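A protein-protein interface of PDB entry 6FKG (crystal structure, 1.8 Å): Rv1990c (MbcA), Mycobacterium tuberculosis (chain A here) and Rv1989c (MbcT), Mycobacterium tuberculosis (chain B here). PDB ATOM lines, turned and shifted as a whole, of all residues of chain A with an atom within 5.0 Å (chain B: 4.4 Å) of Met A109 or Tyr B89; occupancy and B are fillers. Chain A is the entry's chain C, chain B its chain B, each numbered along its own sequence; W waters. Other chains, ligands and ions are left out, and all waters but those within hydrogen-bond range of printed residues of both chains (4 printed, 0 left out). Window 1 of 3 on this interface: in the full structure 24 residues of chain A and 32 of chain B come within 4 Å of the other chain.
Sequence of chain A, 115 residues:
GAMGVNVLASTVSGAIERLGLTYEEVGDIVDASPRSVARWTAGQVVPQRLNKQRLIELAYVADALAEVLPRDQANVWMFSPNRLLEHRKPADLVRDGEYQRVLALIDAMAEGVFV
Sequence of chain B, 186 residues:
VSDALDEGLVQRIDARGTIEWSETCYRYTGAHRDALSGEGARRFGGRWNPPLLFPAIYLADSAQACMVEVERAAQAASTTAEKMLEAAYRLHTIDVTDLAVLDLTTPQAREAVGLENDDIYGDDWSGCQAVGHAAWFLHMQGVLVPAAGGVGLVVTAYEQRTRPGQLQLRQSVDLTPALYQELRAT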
ATOM      1  N   GLU A  67     -23.811 -26.672   5.277  1.00  0.00           N
ATOM      2  CA  GLU A  67     -23.792 -27.566   6.423  1.00  0.00           C
ATOM      3  C   GLU A  67     -22.888 -27.059   7.555  1.00  0.00           C
ATOM      4  O   GLU A  67     -23.063 -27.440   8.706  1.00  0.00           O
ATOM      5  CB  GLU A  67     -23.344 -28.975   6.002  1.00  0.00           C
ATOM      6  CG  GLU A  67     -23.605 -30.022   7.091  1.00  0.00           C
ATOM      7  CD  GLU A  67     -23.091 -31.423   6.741  1.00  0.00           C
ATOM      8  OE1 GLU A  67     -22.454 -31.582   5.674  1.00  0.00           O
ATOM      9  OE2 GLU A  67     -23.333 -32.365   7.541  1.00  0.00           O
ATOM     10  N   VAL A  68     -21.913 -26.211   7.237  1.00  0.00           N
ATOM     11  CA  VAL A  68     -20.863 -25.927   8.214  1.00  0.00           C
ATOM     12  C   VAL A  68     -20.729 -24.438   8.525  1.00  0.00           C
ATOM     13  O   VAL A  68     -20.114 -24.079   9.521  1.00  0.00           O
ATOM     14  CB  VAL A  68     -19.486 -26.478   7.751  1.00  0.00           C
ATOM     15  CG1 VAL A  68     -19.541 -27.997   7.621  1.00  0.00           C
ATOM     16  CG2 VAL A  68     -19.054 -25.876   6.408  1.00  0.00           C
ATOM     17  N   LEU A  69     -21.288 -23.570   7.683  1.00  0.00           N
ATOM     18  CA  LEU A  69     -21.276 -22.125   7.983  1.00  0.00           C
ATOM     19  C   LEU A  69     -22.591 -21.457   7.649  1.00  0.00           C
ATOM     20  O   LEU A  69     -23.193 -21.759   6.628  1.00  0.00           O
ATOM     21  CB  LEU A  69     -20.179 -21.404   7.212  1.00  0.00           C
ATOM     22  CG  LEU A  69     -18.737 -21.684   7.602  1.00  0.00           C
ATOM     23  CD1 LEU A  69     -17.847 -21.023   6.561  1.00  0.00           C
ATOM     24  CD2 LEU A  69     -18.452 -21.165   9.024  1.00  0.00           C
ATOM     25  N   TRP A  77     -16.291 -16.686   3.408  1.00  0.00           N
ATOM     26  CA  TRP A  77     -15.361 -17.829   3.321  1.00  0.00           C
ATOM     27  C   TRP A  77     -14.950 -18.161   1.886  1.00  0.00           C
ATOM     28  O   TRP A  77     -13.793 -18.511   1.624  1.00  0.00           O
ATOM     29  CB  TRP A  77     -16.017 -19.050   3.963  1.00  0.00           C
ATOM     30  CG  TRP A  77     -15.182 -20.272   4.080  1.00  0.00           C
ATOM     31  CD1 TRP A  77     -14.350 -20.603   5.120  1.00  0.00           C
ATOM     32  CD2 TRP A  77     -15.147 -21.383   3.164  1.00  0.00           C
ATOM     33  NE1 TRP A  77     -13.786 -21.848   4.889  1.00  0.00           N
ATOM     34  CE2 TRP A  77     -14.254 -22.337   3.696  1.00  0.00           C
ATOM     35  CE3 TRP A  77     -15.760 -21.644   1.931  1.00  0.00           C
ATOM     36  CZ2 TRP A  77     -13.971 -23.545   3.047  1.00  0.00           C
ATOM     37  CZ3 TRP A  77     -15.483 -22.853   1.289  1.00  0.00           C
ATOM     38  CH2 TRP A  77     -14.602 -23.784   1.851  1.00  0.00           C
ATOM     39  N   LEU A 105     -12.381 -30.298   2.070  1.00  0.00           N
ATOM     40  CA  LEU A 105     -12.208 -29.409   3.231  1.00  0.00           C
ATOM     41  C   LEU A 105     -13.541 -29.222   3.997  1.00  0.00           C
ATOM     42  O   LEU A 105     -13.574 -29.298   5.219  1.00  0.00           O
ATOM     43  CB  LEU A 105     -11.636 -28.045   2.804  1.00  0.00           C
ATOM     44  CG  LEU A 105     -11.584 -26.971   3.907  1.00  0.00           C
ATOM     45  CD1 LEU A 105     -10.851 -27.477   5.137  1.00  0.00           C
ATOM     46  CD2 LEU A 105     -10.932 -25.684   3.403  1.00  0.00           C
ATOM     47  N   ILE A 106     -14.644 -29.015   3.284  1.00  0.00           N
ATOM     48  CA  ILE A 106     -15.950 -28.858   3.937  1.00  0.00           C
ATOM     49  C   ILE A 106     -16.322 -30.108   4.739  1.00  0.00           C
ATOM     50  O   ILE A 106     -16.823 -30.027   5.868  1.00  0.00           O
ATOM     51  CB  ILE A 106     -17.032 -28.507   2.891  1.00  0.00           C
ATOM     52  CG1 ILE A 106     -16.775 -27.087   2.371  1.00  0.00           C
ATOM     53  CG2 ILE A 106     -18.446 -28.654   3.460  1.00  0.00           C
ATOM     54  CD1 ILE A 106     -17.530 -26.754   1.061  1.00  0.00           C
ATOM     55  N   ASP A 107     -16.033 -31.279   4.188  1.00  0.00           N
ATOM     56  CA  ASP A 107     -16.268 -32.523   4.922  1.00  0.00           C
ATOM     57  C   ASP A 107     -15.434 -32.609   6.203  1.00  0.00           C
ATOM     58  O   ASP A 107     -15.929 -33.045   7.242  1.00  0.00           O
ATOM     59  CB  ASP A 107     -15.961 -33.727   4.030  1.00  0.00           C
ATOM     60  CG  ASP A 107     -17.179 -34.234   3.318  1.00  0.00           C
ATOM     61  OD1 ASP A 107     -18.270 -34.188   3.921  1.00  0.00           O
ATOM     62  OD2 ASP A 107     -17.042 -34.694   2.165  1.00  0.00           O
ATOM     63  N   ALA A 108     -14.176 -32.178   6.128  1.00  0.00           N
ATOM     64  CA  ALA A 108     -13.319 -32.143   7.311  1.00  0.00           C
ATOM     65  C   ALA A 108     -13.871 -31.160   8.348  1.00  0.00           C
ATOM     66  O   ALA A 108     -13.879 -31.450   9.535  1.00  0.00           O
ATOM     67  CB  ALA A 108     -11.859 -31.786   6.929  1.00  0.00           C
ATOM     68  N   MET A 109     -14.366 -30.019   7.888  1.00  0.00           N
ATOM     69  CA  MET A 109     -15.007 -29.045   8.777  1.00  0.00           C
ATOM     70  C   MET A 109     -16.218 -29.649   9.485  1.00  0.00           C
ATOM     71  O   MET A 109     -16.401 -29.500  10.696  1.00  0.00           O
ATOM     72  CB  MET A 109     -15.417 -27.814   7.975  1.00  0.00           C
ATOM     73  CG  MET A 109     -14.214 -27.042   7.458  1.00  0.00           C
ATOM     74  SD  MET A 109     -14.696 -25.767   6.293  1.00  0.00           S
ATOM     75  CE  MET A 109     -15.609 -24.678   7.387  1.00  0.00           C
ATOM     76  N   ALA A 110     -17.021 -30.372   8.722  1.00  0.00           N
ATOM     77  CA  ALA A 110     -18.218 -31.003   9.239  1.00  0.00           C
ATOM     78  C   ALA A 110     -17.904 -32.137  10.219  1.00  0.00           C
ATOM     79  O   ALA A 110     -18.773 -32.545  10.997  1.00  0.00           O
ATOM     80  CB  ALA A 110     -19.078 -31.537   8.070  1.00  0.00           C
ATOM     81  N   GLU A 111     -16.685 -32.677  10.161  1.00  0.00           N
ATOM     82  CA  GLU A 111     -16.297 -33.741  11.084  1.00  0.00           C
ATOM     83  C   GLU A 111     -15.400 -33.265  12.216  1.00  0.00           C
ATOM     84  O   GLU A 111     -14.838 -34.073  12.953  1.00  0.00           O
ATOM     85  CB  GLU A 111     -15.612 -34.878  10.326  1.00  0.00           C
ATOM     86  CG  GLU A 111     -16.580 -35.533   9.377  1.00  0.00           C
ATOM     87  CD  GLU A 111     -16.272 -36.986   9.117  1.00  0.00           C
ATOM     88  OE1 GLU A 111     -15.227 -37.476   9.588  1.00  0.00           O
ATOM     89  OE2 GLU A 111     -17.099 -37.632   8.449  1.00  0.00           O
ATOM     90  N   GLY A 112     -15.272 -31.952  12.355  1.00  0.00           N
ATOM     91  CA  GLY A 112     -14.509 -31.394  13.468  1.00  0.00           C
ATOM     92  C   GLY A 112     -13.052 -31.831  13.477  1.00  0.00           C
ATOM     93  O   GLY A 112     -12.456 -32.058  14.522  1.00  0.00           O
ATOM     94  N   VAL A 113     -12.469 -31.955  12.292  1.00  0.00           N
ATOM     95  CA  VAL A 113     -11.055 -32.278  12.183  1.00  0.00           C
ATOM     96  C   VAL A 113     -10.210 -31.163  12.788  1.00  0.00           C
ATOM     97  O   VAL A 113     -10.464 -29.990  12.508  1.00  0.00           O
ATOM     98  CB  VAL A 113     -10.666 -32.498  10.705  1.00  0.00           C
ATOM     99  CG1 VAL A 113      -9.162 -32.696  10.576  1.00  0.00           C
ATOM    100  CG2 VAL A 113     -11.440 -33.701  10.138  1.00  0.00           C
ATOM    101  N   TYR B  28     -16.574 -32.612  18.256  1.00  0.00           N
ATOM    102  CA  TYR B  28     -17.726 -31.912  17.687  1.00  0.00           C
ATOM    103  C   TYR B  28     -17.837 -32.256  16.198  1.00  0.00           C
ATOM    104  O   TYR B  28     -16.846 -32.579  15.533  1.00  0.00           O
ATOM    105  CB  TYR B  28     -17.646 -30.374  17.931  1.00  0.00           C
ATOM    106  CG  TYR B  28     -16.673 -29.663  17.019  1.00  0.00           C
ATOM    107  CD1 TYR B  28     -15.308 -29.734  17.243  1.00  0.00           C
ATOM    108  CD2 TYR B  28     -17.122 -28.923  15.933  1.00  0.00           C
ATOM    109  CE1 TYR B  28     -14.412 -29.108  16.404  1.00  0.00           C
ATOM    110  CE2 TYR B  28     -16.227 -28.296  15.079  1.00  0.00           C
ATOM    111  CZ  TYR B  28     -14.879 -28.392  15.320  1.00  0.00           C
ATOM    112  OH  TYR B  28     -13.989 -27.761  14.475  1.00  0.00           O
ATOM    113  N   THR B  29     -19.072 -32.277  15.699  1.00  0.00           N
ATOM    114  CA  THR B  29     -19.332 -32.534  14.294  1.00  0.00           C
ATOM    115  C   THR B  29     -20.540 -31.705  13.903  1.00  0.00           C
ATOM    116  O   THR B  29     -21.282 -31.237  14.767  1.00  0.00           O
ATOM    117  CB  THR B  29     -19.669 -34.028  13.987  1.00  0.00           C
ATOM    118  OG1 THR B  29     -20.925 -34.364  14.585  1.00  0.00           O
ATOM    119  CG2 THR B  29     -18.580 -34.970  14.476  1.00  0.00           C
ATOM    120  N   GLY B  30     -20.760 -31.551  12.605  1.00  0.00           N
ATOM    121  CA  GLY B  30     -22.070 -31.142  12.132  1.00  0.00           C
ATOM    122  C   GLY B  30     -23.120 -32.060  12.722  1.00  0.00           C
ATOM    123  O   GLY B  30     -22.854 -33.250  12.985  1.00  0.00           O
ATOM    124  N   ALA B  31     -24.316 -31.513  12.916  1.00  0.00           N
ATOM    125  CA  ALA B  31     -25.383 -32.201  13.629  1.00  0.00           C
ATOM    126  C   ALA B  31     -25.833 -33.478  12.918  1.00  0.00           C
ATOM    127  O   ALA B  31     -26.381 -34.384  13.549  1.00  0.00           O
ATOM    128  CB  ALA B  31     -26.574 -31.259  13.825  1.00  0.00           C
ATOM    129  N   ALA B  77     -11.517 -20.626   9.200  1.00  0.00           N
ATOM    130  CA  ALA B  77     -12.663 -20.337   8.346  1.00  0.00           C
ATOM    131  C   ALA B  77     -12.987 -18.838   8.340  1.00  0.00           C
ATOM    132  O   ALA B  77     -14.058 -18.445   7.903  1.00  0.00           O
ATOM    133  CB  ALA B  77     -13.872 -21.133   8.808  1.00  0.00           C
ATOM    134  N   MET B  84     -19.823 -19.371  13.763  1.00  0.00           N
ATOM    135  CA  MET B  84     -19.785 -20.673  13.083  1.00  0.00           C
ATOM    136  C   MET B  84     -20.858 -21.604  13.621  1.00  0.00           C
ATOM    137  O   MET B  84     -21.497 -22.358  12.860  1.00  0.00           O
ATOM    138  CB  MET B  84     -18.406 -21.323  13.236  1.00  0.00           C
ATOM    139  CG  MET B  84     -18.243 -22.656  12.509  1.00  0.00           C
ATOM    140  SD  MET B  84     -16.535 -23.244  12.627  1.00  0.00           S
ATOM    141  CE  MET B  84     -16.624 -24.240  14.095  1.00  0.00           C
ATOM    142  N   LEU B  85     -21.065 -21.540  14.934  1.00  0.00           N
ATOM    143  CA  LEU B  85     -22.008 -22.435  15.605  1.00  0.00           C
ATOM    144  C   LEU B  85     -23.468 -22.021  15.414  1.00  0.00           C
ATOM    145  O   LEU B  85     -24.369 -22.610  16.004  1.00  0.00           O
ATOM    146  CB  LEU B  85     -21.681 -22.518  17.083  1.00  0.00           C
ATOM    147  CG  LEU B  85     -20.364 -23.244  17.377  1.00  0.00           C
ATOM    148  CD1 LEU B  85     -20.040 -23.139  18.854  1.00  0.00           C
ATOM    149  CD2 LEU B  85     -20.442 -24.729  16.933  1.00  0.00           C
ATOM    150  N   ALA B  87     -24.500 -22.393  12.421  1.00  0.00           N
ATOM    151  CA  ALA B  87     -24.779 -23.610  11.648  1.00  0.00           C
ATOM    152  C   ALA B  87     -24.887 -24.743  12.670  1.00  0.00           C
ATOM    153  O   ALA B  87     -24.373 -24.622  13.781  1.00  0.00           O
ATOM    154  CB  ALA B  87     -23.683 -23.881  10.608  1.00  0.00           C
ATOM    155  N   ALA B  88     -25.581 -25.823  12.318  1.00  0.00           N
ATOM    156  CA  ALA B  88     -25.936 -26.848  13.297  1.00  0.00           C
ATOM    157  C   ALA B  88     -24.787 -27.809  13.600  1.00  0.00           C
ATOM    158  O   ALA B  88     -24.434 -28.651  12.768  1.00  0.00           O
ATOM    159  CB  ALA B  88     -27.148 -27.625  12.812  1.00  0.00           C
ATOM    160  N   TYR B  89     -24.219 -27.693  14.797  1.00  0.00           N
ATOM    161  CA  TYR B  89     -23.195 -28.631  15.257  1.00  0.00           C
ATOM    162  C   TYR B  89     -23.647 -29.343  16.527  1.00  0.00           C
ATOM    163  O   TYR B  89     -24.525 -28.867  17.251  1.00  0.00           O
ATOM    164  CB  TYR B  89     -21.871 -27.921  15.549  1.00  0.00           C
ATOM    165  CG  TYR B  89     -21.130 -27.428  14.331  1.00  0.00           C
ATOM    166  CD1 TYR B  89     -21.408 -26.181  13.782  1.00  0.00           C
ATOM    167  CD2 TYR B  89     -20.144 -28.209  13.739  1.00  0.00           C
ATOM    168  CE1 TYR B  89     -20.709 -25.724  12.659  1.00  0.00           C
ATOM    169  CE2 TYR B  89     -19.448 -27.775  12.613  1.00  0.00           C
ATOM    170  CZ  TYR B  89     -19.726 -26.524  12.089  1.00  0.00           C
ATOM    171  OH  TYR B  89     -19.034 -26.083  10.984  1.00  0.00           O
ATOM    172  N   ARG B  90     -23.025 -30.481  16.805  1.00  0.00           N
ATOM    173  CA  ARG B  90     -23.291 -31.203  18.039  1.00  0.00           C
ATOM    174  C   ARG B  90     -21.989 -31.572  18.741  1.00  0.00           C
ATOM    175  O   ARG B  90     -20.945 -31.746  18.098  1.00  0.00           O
ATOM    176  CB  ARG B  90     -24.140 -32.452  17.764  1.00  0.00           C
ATOM    177  CG  ARG B  90     -25.591 -32.115  17.413  1.00  0.00           C
ATOM    178  CD  ARG B  90     -26.471 -33.349  17.353  1.00  0.00           C
ATOM    179  NE  ARG B  90     -27.881 -33.004  17.199  1.00  0.00           N
ATOM    180  CZ  ARG B  90     -28.809 -33.852  16.773  1.00  0.00           C
ATOM    181  NH1 ARG B  90     -30.072 -33.461  16.661  1.00  0.00           N
ATOM    182  NH2 ARG B  90     -28.469 -35.093  16.452  1.00  0.00           N
ATOM    183  N   VAL B 173     -25.118 -33.466  22.279  1.00  0.00           N
ATOM    184  CA  VAL B 173     -25.969 -32.311  22.554  1.00  0.00           C
ATOM    185  C   VAL B 173     -25.747 -31.257  21.488  1.00  0.00           C
ATOM    186  O   VAL B 173     -24.694 -31.226  20.868  1.00  0.00           O
ATOM    187  CB  VAL B 173     -25.695 -31.688  23.949  1.00  0.00           C
ATOM    188  CG1 VAL B 173     -26.028 -32.695  25.048  1.00  0.00           C
ATOM    189  CG2 VAL B 173     -24.243 -31.195  24.050  1.00  0.00           C
ATOM    190  N   ASP B 174     -26.732 -30.390  21.284  1.00  0.00           N
ATOM    191  CA  ASP B 174     -26.574 -29.315  20.314  1.00  0.00           C
ATOM    192  C   ASP B 174     -25.538 -28.328  20.804  1.00  0.00           C
ATOM    193  O   ASP B 174     -25.617 -27.840  21.939  1.00  0.00           O
ATOM    194  CB  ASP B 174     -27.893 -28.606  20.051  1.00  0.00           C
ATOM    195  CG  ASP B 174     -28.910 -29.503  19.359  1.00  0.00           C
ATOM    196  OD1 ASP B 174     -28.509 -30.502  18.728  1.00  0.00           O
ATOM    197  OD2 ASP B 174     -30.106 -29.185  19.430  1.00  0.00           O
ATOM    198  N   LEU B 175     -24.556 -28.034  19.961  1.00  0.00           N
ATOM    199  CA  LEU B 175     -23.480 -27.131  20.367  1.00  0.00           C
ATOM    200  C   LEU B 175     -23.801 -25.727  19.877  1.00  0.00           C
ATOM    201  O   LEU B 175     -23.380 -25.307  18.803  1.00  0.00           O
ATOM    202  CB  LEU B 175     -22.128 -27.607  19.840  1.00  0.00           C
ATOM    203  CG  LEU B 175     -20.897 -26.801  20.290  1.00  0.00           C
ATOM    204  CD1 LEU B 175     -20.751 -26.739  21.822  1.00  0.00           C
ATOM    205  CD2 LEU B 175     -19.664 -27.407  19.643  1.00  0.00           C
HETATM  206  O   HOH W   1     -24.295 -31.654   9.843  1.00  0.00           O
HETATM  207  O   HOH W   2     -13.669 -32.846  17.010  1.00  0.00           O
HETATM  208  O   HOH W   3     -14.928 -27.646  11.907  1.00  0.00           O
HETATM  209  O   HOH W   4     -11.332 -28.556  14.626  1.00  0.00           O
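Val A68 touches Met B84 (O to CG, 3.8 Å).
CB of Ala B87 touches C of Val A68, 3.7 Å away.
Leu A69 touches Met B84.
Ala B87 touches Leu A69.
Trp A77 touches Ala B77.
Tyr B89 touches Met A109.
O of Ala A110 touches CA of Thr B29, 3.3 Å away.
Glu A111 touches Tyr B28.
Gly A112 touches Tyr B28.
Water W1 bridges OE2 of Glu A67 (2.6 Å) and N of Ala B31 (3.1 Å).
Water W3 lies within hydrogen-bond range of O of Met A109 and OH of Tyr B28.
Water W4 lies within hydrogen-bond range of the backbone carbonyl oxygen of Val A113 (2.7 Å) and the side-chain hydroxyl of Tyr B28 (2.8 Å).
Water W2 lies within hydrogen-bond range of O of Gly A112 (2.9 Å) and N of Tyr B28 (3.2 Å).
The backbone carbonyl oxygen (O) of Ala A110 sits at hydrogen-bond distance from the backbone NH (N) of Gly B30 (2.7 Å).
The side-chain hydroxyl of Tyr B89 lies within hydrogen-bond range of the backbone carbonyl oxygen of Val A68 (2.7 Å).
Of the 14 printed residues of chain B, 7 touch a printed residue of chain A.
Along chain B the printed residues that touch a printed residue of chain A span positions 28 to 89.
Of the 13 printed residues of chain A, 7 touch a printed residue of chain B.
Printed residues of chain A that touch a printed residue of chain B: Val A68, Leu A69, Trp A77, Met A109, Ala A110, Glu A111 and Gly A112.
Among the printed residues, 11 pairs touch across the chains.
The backbone NH (N) of Arg B90 sits at hydrogen-bond distance from the backbone carbonyl oxygen (O) of Thr B29 (2.8 Å).
O of Tyr B89 lies within hydrogen-bond range of N of Leu B175.
Of the printed residues of chain B, Met A109 touches Tyr B89.
Printed residues of chain A within 4 Å of Tyr B89: Val A68 (2.7 Å) and Met A109 (3.99 Å).
Printed residues of chain A within 4 Å of Met B84: Val A68 and Leu A69.
Printed residues of chain A within 4 Å of Ala B77: Trp A77 (3.5 Å).
Of the printed residues of chain B, Ala A110 touches Thr B29 (3.3 Å) and Gly B30 (2.7 Å).
The nearest printed residue of chain A that does not touch Tyr B89 is Leu A69 (4.7 Å).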
